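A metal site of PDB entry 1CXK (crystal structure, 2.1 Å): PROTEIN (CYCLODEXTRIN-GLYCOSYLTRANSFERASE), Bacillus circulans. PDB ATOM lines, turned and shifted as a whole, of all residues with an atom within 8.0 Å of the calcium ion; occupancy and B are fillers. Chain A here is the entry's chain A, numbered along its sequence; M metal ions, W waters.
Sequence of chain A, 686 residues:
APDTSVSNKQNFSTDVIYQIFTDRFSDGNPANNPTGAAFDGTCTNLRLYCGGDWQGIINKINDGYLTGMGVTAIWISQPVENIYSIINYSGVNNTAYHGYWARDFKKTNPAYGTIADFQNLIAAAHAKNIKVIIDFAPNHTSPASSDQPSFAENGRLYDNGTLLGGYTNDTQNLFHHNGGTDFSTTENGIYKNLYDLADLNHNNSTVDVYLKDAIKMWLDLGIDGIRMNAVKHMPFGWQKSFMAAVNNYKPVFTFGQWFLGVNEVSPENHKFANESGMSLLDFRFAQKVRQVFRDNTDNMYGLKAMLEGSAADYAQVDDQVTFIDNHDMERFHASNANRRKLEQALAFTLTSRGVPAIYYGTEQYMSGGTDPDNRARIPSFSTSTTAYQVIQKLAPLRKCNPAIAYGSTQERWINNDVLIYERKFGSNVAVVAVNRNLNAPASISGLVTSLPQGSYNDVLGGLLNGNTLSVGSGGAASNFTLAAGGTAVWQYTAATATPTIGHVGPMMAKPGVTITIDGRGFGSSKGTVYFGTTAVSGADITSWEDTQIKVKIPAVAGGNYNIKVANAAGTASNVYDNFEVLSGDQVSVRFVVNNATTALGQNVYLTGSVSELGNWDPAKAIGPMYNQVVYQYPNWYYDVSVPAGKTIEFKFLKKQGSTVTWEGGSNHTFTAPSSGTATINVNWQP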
ATOM      1  N   THR A  22     -33.748   9.022 -11.890  1.00  0.00           N
ATOM      2  CA  THR A  22     -33.395  10.210 -11.138  1.00  0.00           C
ATOM      3  C   THR A  22     -31.930  10.427 -10.805  1.00  0.00           C
ATOM      4  O   THR A  22     -31.379  11.487 -11.076  1.00  0.00           O
ATOM      5  CB  THR A  22     -34.306  10.405  -9.923  1.00  0.00           C
ATOM      6  OG1 THR A  22     -35.651  10.215 -10.321  1.00  0.00           O
ATOM      7  CG2 THR A  22     -34.117  11.801  -9.333  1.00  0.00           C
ATOM      8  N   ASP A  23     -31.297   9.414 -10.230  1.00  0.00           N
ATOM      9  CA  ASP A  23     -29.908   9.525  -9.843  1.00  0.00           C
ATOM     10  C   ASP A  23     -28.931   9.737 -10.995  1.00  0.00           C
ATOM     11  O   ASP A  23     -27.849  10.281 -10.796  1.00  0.00           O
ATOM     12  CB  ASP A  23     -29.455   8.322  -9.000  1.00  0.00           C
ATOM     13  CG  ASP A  23     -28.084   8.526  -8.408  1.00  0.00           C
ATOM     14  OD1 ASP A  23     -27.834   9.413  -7.615  1.00  0.00           O
ATOM     15  OD2 ASP A  23     -27.191   7.670  -8.867  1.00  0.00           O
ATOM     16  N   SER A  26     -29.663  14.344 -13.583  1.00  0.00           N
ATOM     17  CA  SER A  26     -29.000  15.606 -13.324  1.00  0.00           C
ATOM     18  C   SER A  26     -28.953  16.004 -11.864  1.00  0.00           C
ATOM     19  O   SER A  26     -29.986  16.173 -11.216  1.00  0.00           O
ATOM     20  CB  SER A  26     -29.623  16.697 -14.169  1.00  0.00           C
ATOM     21  OG  SER A  26     -29.003  17.938 -13.896  1.00  0.00           O
ATOM     22  N   ASP A  27     -27.748  16.176 -11.347  1.00  0.00           N
ATOM     23  CA  ASP A  27     -27.556  16.573  -9.970  1.00  0.00           C
ATOM     24  C   ASP A  27     -27.699  18.085  -9.854  1.00  0.00           C
ATOM     25  O   ASP A  27     -26.731  18.810 -10.049  1.00  0.00           O
ATOM     26  CB  ASP A  27     -26.199  16.109  -9.430  1.00  0.00           C
ATOM     27  CG  ASP A  27     -25.873  16.629  -8.066  1.00  0.00           C
ATOM     28  OD1 ASP A  27     -26.689  17.105  -7.305  1.00  0.00           O
ATOM     29  OD2 ASP A  27     -24.603  16.476  -7.772  1.00  0.00           O
ATOM     30  N   GLY A  28     -28.919  18.543  -9.559  1.00  0.00           N
ATOM     31  CA  GLY A  28     -29.178  19.977  -9.442  1.00  0.00           C
ATOM     32  C   GLY A  28     -28.945  20.522  -8.037  1.00  0.00           C
ATOM     33  O   GLY A  28     -28.986  21.728  -7.833  1.00  0.00           O
ATOM     34  N   ASN A  29     -28.705  19.635  -7.078  1.00  0.00           N
ATOM     35  CA  ASN A  29     -28.459  20.025  -5.700  1.00  0.00           C
ATOM     36  C   ASN A  29     -27.436  19.126  -5.024  1.00  0.00           C
ATOM     37  O   ASN A  29     -27.760  18.144  -4.357  1.00  0.00           O
ATOM     38  CB  ASN A  29     -29.743  20.122  -4.853  1.00  0.00           C
ATOM     39  CG  ASN A  29     -29.464  20.605  -3.433  1.00  0.00           C
ATOM     40  OD1 ASN A  29     -28.325  20.961  -3.095  1.00  0.00           O
ATOM     41  ND2 ASN A  29     -30.508  20.635  -2.610  1.00  0.00           N
ATOM     42  N   PRO A  30     -26.173  19.477  -5.229  1.00  0.00           N
ATOM     43  CA  PRO A  30     -25.061  18.725  -4.674  1.00  0.00           C
ATOM     44  C   PRO A  30     -25.110  18.604  -3.165  1.00  0.00           C
ATOM     45  O   PRO A  30     -24.552  17.670  -2.582  1.00  0.00           O
ATOM     46  CB  PRO A  30     -23.792  19.453  -5.112  1.00  0.00           C
ATOM     47  CG  PRO A  30     -24.198  20.559  -6.069  1.00  0.00           C
ATOM     48  CD  PRO A  30     -25.716  20.595  -6.094  1.00  0.00           C
ATOM     49  N   ALA A  31     -25.797  19.555  -2.523  1.00  0.00           N
ATOM     50  CA  ALA A  31     -25.915  19.576  -1.078  1.00  0.00           C
ATOM     51  C   ALA A  31     -26.651  18.365  -0.523  1.00  0.00           C
ATOM     52  O   ALA A  31     -26.467  17.990   0.622  1.00  0.00           O
ATOM     53  CB  ALA A  31     -26.576  20.865  -0.616  1.00  0.00           C
ATOM     54  N   ASN A  32     -27.497  17.761  -1.347  1.00  0.00           N
ATOM     55  CA  ASN A  32     -28.235  16.601  -0.884  1.00  0.00           C
ATOM     56  C   ASN A  32     -27.569  15.286  -1.251  1.00  0.00           C
ATOM     57  O   ASN A  32     -28.088  14.213  -0.950  1.00  0.00           O
ATOM     58  CB  ASN A  32     -29.722  16.635  -1.271  1.00  0.00           C
ATOM     59  CG  ASN A  32     -29.945  16.591  -2.769  1.00  0.00           C
ATOM     60  OD1 ASN A  32     -29.144  16.005  -3.501  1.00  0.00           O
ATOM     61  ND2 ASN A  32     -31.032  17.208  -3.211  1.00  0.00           N
ATOM     62  N   ASN A  33     -26.417  15.367  -1.919  1.00  0.00           N
ATOM     63  CA  ASN A  33     -25.721  14.160  -2.310  1.00  0.00           C
ATOM     64  C   ASN A  33     -25.328  13.313  -1.122  1.00  0.00           C
ATOM     65  O   ASN A  33     -24.917  13.841  -0.096  1.00  0.00           O
ATOM     66  CB  ASN A  33     -24.435  14.475  -3.106  1.00  0.00           C
ATOM     67  CG  ASN A  33     -24.695  15.154  -4.427  1.00  0.00           C
ATOM     68  OD1 ASN A  33     -25.858  15.276  -4.863  1.00  0.00           O
ATOM     69  ND2 ASN A  33     -23.625  15.584  -5.083  1.00  0.00           N
ATOM     70  N   PRO A  34     -25.425  11.995  -1.290  1.00  0.00           N
ATOM     71  CA  PRO A  34     -25.004  11.100  -0.225  1.00  0.00           C
ATOM     72  C   PRO A  34     -23.485  11.203  -0.125  1.00  0.00           C
ATOM     73  O   PRO A  34     -22.823  11.658  -1.058  1.00  0.00           O
ATOM     74  CB  PRO A  34     -25.463   9.698  -0.638  1.00  0.00           C
ATOM     75  CG  PRO A  34     -26.531   9.890  -1.705  1.00  0.00           C
ATOM     76  CD  PRO A  34     -26.406  11.330  -2.184  1.00  0.00           C
ATOM     77  N   PHE A  39     -21.139   7.136  -2.368  1.00  0.00           N
ATOM     78  CA  PHE A  39     -21.180   8.072  -3.485  1.00  0.00           C
ATOM     79  C   PHE A  39     -19.971   8.110  -4.399  1.00  0.00           C
ATOM     80  O   PHE A  39     -18.827   7.985  -3.985  1.00  0.00           O
ATOM     81  CB  PHE A  39     -21.390   9.466  -2.860  1.00  0.00           C
ATOM     82  CG  PHE A  39     -21.526  10.583  -3.860  1.00  0.00           C
ATOM     83  CD1 PHE A  39     -22.752  10.824  -4.495  1.00  0.00           C
ATOM     84  CD2 PHE A  39     -20.451  11.429  -4.151  1.00  0.00           C
ATOM     85  CE1 PHE A  39     -22.889  11.867  -5.407  1.00  0.00           C
ATOM     86  CE2 PHE A  39     -20.571  12.469  -5.058  1.00  0.00           C
ATOM     87  CZ  PHE A  39     -21.804  12.685  -5.683  1.00  0.00           C
ATOM     88  N   TYR A  49     -24.497   6.062  -5.569  1.00  0.00           N
ATOM     89  CA  TYR A  49     -25.250   7.248  -5.947  1.00  0.00           C
ATOM     90  C   TYR A  49     -24.367   8.181  -6.748  1.00  0.00           C
ATOM     91  O   TYR A  49     -23.212   8.397  -6.375  1.00  0.00           O
ATOM     92  CB  TYR A  49     -25.788   8.041  -4.727  1.00  0.00           C
ATOM     93  CG  TYR A  49     -27.082   7.566  -4.122  1.00  0.00           C
ATOM     94  CD1 TYR A  49     -27.080   6.637  -3.076  1.00  0.00           C
ATOM     95  CD2 TYR A  49     -28.309   8.075  -4.536  1.00  0.00           C
ATOM     96  CE1 TYR A  49     -28.268   6.209  -2.478  1.00  0.00           C
ATOM     97  CE2 TYR A  49     -29.519   7.661  -3.959  1.00  0.00           C
ATOM     98  CZ  TYR A  49     -29.487   6.721  -2.919  1.00  0.00           C
ATOM     99  OH  TYR A  49     -30.650   6.305  -2.335  1.00  0.00           O
ATOM    100  N   CYS A  50     -24.897   8.747  -7.829  1.00  0.00           N
ATOM    101  CA  CYS A  50     -24.134   9.667  -8.644  1.00  0.00           C
ATOM    102  C   CYS A  50     -24.503  11.107  -8.352  1.00  0.00           C
ATOM    103  O   CYS A  50     -23.763  12.020  -8.685  1.00  0.00           O
ATOM    104  CB  CYS A  50     -24.183   9.341 -10.141  1.00  0.00           C
ATOM    105  SG  CYS A  50     -23.584   7.664 -10.500  1.00  0.00           S
ATOM    106  N   GLY A  51     -25.672  11.307  -7.719  1.00  0.00           N
ATOM    107  CA  GLY A  51     -26.122  12.643  -7.329  1.00  0.00           C
ATOM    108  C   GLY A  51     -27.365  13.213  -8.016  1.00  0.00           C
ATOM    109  O   GLY A  51     -27.846  14.264  -7.613  1.00  0.00           O
ATOM    110  N   GLY A  52     -27.874  12.541  -9.058  1.00  0.00           N
ATOM    111  CA  GLY A  52     -29.059  13.036  -9.758  1.00  0.00           C
ATOM    112  C   GLY A  52     -30.220  13.290  -8.806  1.00  0.00           C
ATOM    113  O   GLY A  52     -30.479  12.483  -7.907  1.00  0.00           O
ATOM    114  N   ASP A  53     -30.940  14.397  -8.981  1.00  0.00           N
ATOM    115  CA  ASP A  53     -32.042  14.701  -8.080  1.00  0.00           C
ATOM    116  C   ASP A  53     -33.216  15.443  -8.721  1.00  0.00           C
ATOM    117  O   ASP A  53     -33.216  15.752  -9.906  1.00  0.00           O
ATOM    118  CB  ASP A  53     -31.517  15.505  -6.871  1.00  0.00           C
ATOM    119  CG  ASP A  53     -30.789  16.756  -7.291  1.00  0.00           C
ATOM    120  OD1 ASP A  53     -31.105  17.427  -8.274  1.00  0.00           O
ATOM    121  OD2 ASP A  53     -29.768  17.050  -6.513  1.00  0.00           O
ATOM    122  N   TRP A  54     -34.229  15.728  -7.906  1.00  0.00           N
ATOM    123  CA  TRP A  54     -35.417  16.424  -8.356  1.00  0.00           C
ATOM    124  C   TRP A  54     -35.115  17.841  -8.828  1.00  0.00           C
ATOM    125  O   TRP A  54     -35.693  18.316  -9.814  1.00  0.00           O
ATOM    126  CB  TRP A  54     -36.561  16.399  -7.301  1.00  0.00           C
ATOM    127  CG  TRP A  54     -37.062  15.013  -7.027  1.00  0.00           C
ATOM    128  CD1 TRP A  54     -37.003  13.969  -7.884  1.00  0.00           C
ATOM    129  CD2 TRP A  54     -37.665  14.529  -5.828  1.00  0.00           C
ATOM    130  NE1 TRP A  54     -37.545  12.850  -7.297  1.00  0.00           N
ATOM    131  CE2 TRP A  54     -37.949  13.155  -6.029  1.00  0.00           C
ATOM    132  CE3 TRP A  54     -37.980  15.102  -4.593  1.00  0.00           C
ATOM    133  CZ2 TRP A  54     -38.550  12.374  -5.045  1.00  0.00           C
ATOM    134  CZ3 TRP A  54     -38.580  14.328  -3.631  1.00  0.00           C
ATOM    135  CH2 TRP A  54     -38.851  12.975  -3.848  1.00  0.00           C
ATOM    136  N   GLN A  55     -34.216  18.533  -8.142  1.00  0.00           N
ATOM    137  CA  GLN A  55     -33.866  19.876  -8.570  1.00  0.00           C
ATOM    138  C   GLN A  55     -33.296  19.824  -9.977  1.00  0.00           C
ATOM    139  O   GLN A  55     -33.533  20.701 -10.803  1.00  0.00           O
ATOM    140  CB  GLN A  55     -32.900  20.582  -7.602  1.00  0.00           C
ATOM    141  CG  GLN A  55     -32.475  21.984  -8.068  1.00  0.00           C
ATOM    142  CD  GLN A  55     -33.610  22.986  -8.083  1.00  0.00           C
ATOM    143  OE1 GLN A  55     -34.310  23.163  -7.066  1.00  0.00           O
ATOM    144  NE2 GLN A  55     -33.794  23.650  -9.213  1.00  0.00           N
ATOM    145  N   GLY A  56     -32.536  18.761 -10.237  1.00  0.00           N
ATOM    146  CA  GLY A  56     -31.940  18.563 -11.541  1.00  0.00           C
ATOM    147  C   GLY A  56     -33.021  18.456 -12.600  1.00  0.00           C
ATOM    148  O   GLY A  56     -32.942  19.066 -13.662  1.00  0.00           O
ATOM    149  N   PRO A 110     -34.244  11.514   0.749  1.00  0.00           N
ATOM    150  CA  PRO A 110     -33.499  12.759   0.861  1.00  0.00           C
ATOM    151  C   PRO A 110     -32.511  13.019  -0.261  1.00  0.00           C
ATOM    152  O   PRO A 110     -32.212  14.170  -0.576  1.00  0.00           O
ATOM    153  CB  PRO A 110     -32.777  12.742   2.214  1.00  0.00           C
ATOM    154  CG  PRO A 110     -32.934  11.339   2.783  1.00  0.00           C
ATOM    155  CD  PRO A 110     -33.879  10.582   1.860  1.00  0.00           C
ATOM    156  N   ALA A 111     -31.982  11.956  -0.859  1.00  0.00           N
ATOM    157  CA  ALA A 111     -31.032  12.143  -1.955  1.00  0.00           C
ATOM    158  C   ALA A 111     -31.704  12.818  -3.134  1.00  0.00           C
ATOM    159  O   ALA A 111     -31.100  13.641  -3.830  1.00  0.00           O
ATOM    160  CB  ALA A 111     -30.342  10.839  -2.336  1.00  0.00           C
ATOM    161  N   TYR A 112     -32.987  12.474  -3.343  1.00  0.00           N
ATOM    162  CA  TYR A 112     -33.791  13.047  -4.418  1.00  0.00           C
ATOM    163  C   TYR A 112     -34.286  14.432  -4.013  1.00  0.00           C
ATOM    164  O   TYR A 112     -34.338  15.358  -4.822  1.00  0.00           O
ATOM    165  CB  TYR A 112     -34.983  12.159  -4.850  1.00  0.00           C
ATOM    166  CG  TYR A 112     -34.634  10.753  -5.330  1.00  0.00           C
ATOM    167  CD1 TYR A 112     -33.355  10.401  -5.752  1.00  0.00           C
ATOM    168  CD2 TYR A 112     -35.630   9.777  -5.370  1.00  0.00           C
ATOM    169  CE1 TYR A 112     -33.065   9.105  -6.194  1.00  0.00           C
ATOM    170  CE2 TYR A 112     -35.364   8.488  -5.812  1.00  0.00           C
ATOM    171  CZ  TYR A 112     -34.072   8.151  -6.228  1.00  0.00           C
ATOM    172  OH  TYR A 112     -33.811   6.871  -6.648  1.00  0.00           O
ATOM    173  N   GLY A 113     -34.646  14.569  -2.741  1.00  0.00           N
ATOM    174  CA  GLY A 113     -35.122  15.859  -2.245  1.00  0.00           C
ATOM    175  C   GLY A 113     -36.124  15.726  -1.129  1.00  0.00           C
ATOM    176  O   GLY A 113     -36.432  14.627  -0.670  1.00  0.00           O
HETATM  177 CA    CA M   1     -27.877  15.862  -5.590  1.00  0.00          CA
HETATM  178  O   HOH W   1     -28.555  13.695  -4.754  1.00  0.00           O
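ND2 of Asn 33 sits close to O of Pro 30 (3.4 Å).
The backbone NH (N) of Gly 28 sits at hydrogen-bond distance from the side-chain carboxylate (OD1) of Asp 53 (2.8 Å).
The backbone NH (N) of Asp 53 is in hydrogen-bond range of the backbone carbonyl oxygen (O) of Ser 26.
The side-chain carboxylate (OD1) of Asp 53 lies close to the backbone NH (N) of Gln 55 (3.3 Å).
The side-chain carboxylate (OD1) of Asp 53 is in hydrogen-bond range of the backbone NH (N) of Gly 56 (2.8 Å).
OD1 of Asn 32 lies close to O of Ala 111 (3.1 Å).
The side-chain carboxylate of Asp 23 sits at hydrogen-bond distance from the backbone NH of Gly 51.
The side-chain amide oxygen of Asn 29 sits at hydrogen-bond distance from the backbone NH of Ala 31.
Six residues have an atom within 4 Å of the calcium ion: Asp 27, Asn 29, Asn 32, Asn 33, Gly 51 and Asp 53.
The nearest printed residue that does not touch the calcium ion is Pro 30 (4.01 Å).
OD1 of Asn 33 is bound to the calcium ion (2.2 Å).
The calcium ion is bound by OD2 of Asp 53, at 2.4 Å.
Water W1 is bound to the calcium ion, 2.4 Å away.
The side-chain carboxylate (OD1) of Asp 27 is bound to the calcium ion (2.4 Å).
OD1 of Asn 32 binds the calcium ion (2.4 Å).
The calcium ion is bound by O of Gly 51 (2.6 Å).
O of Asn 29 is bound to the calcium ion.
The calcium ion has seven donor atoms within binding distance.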
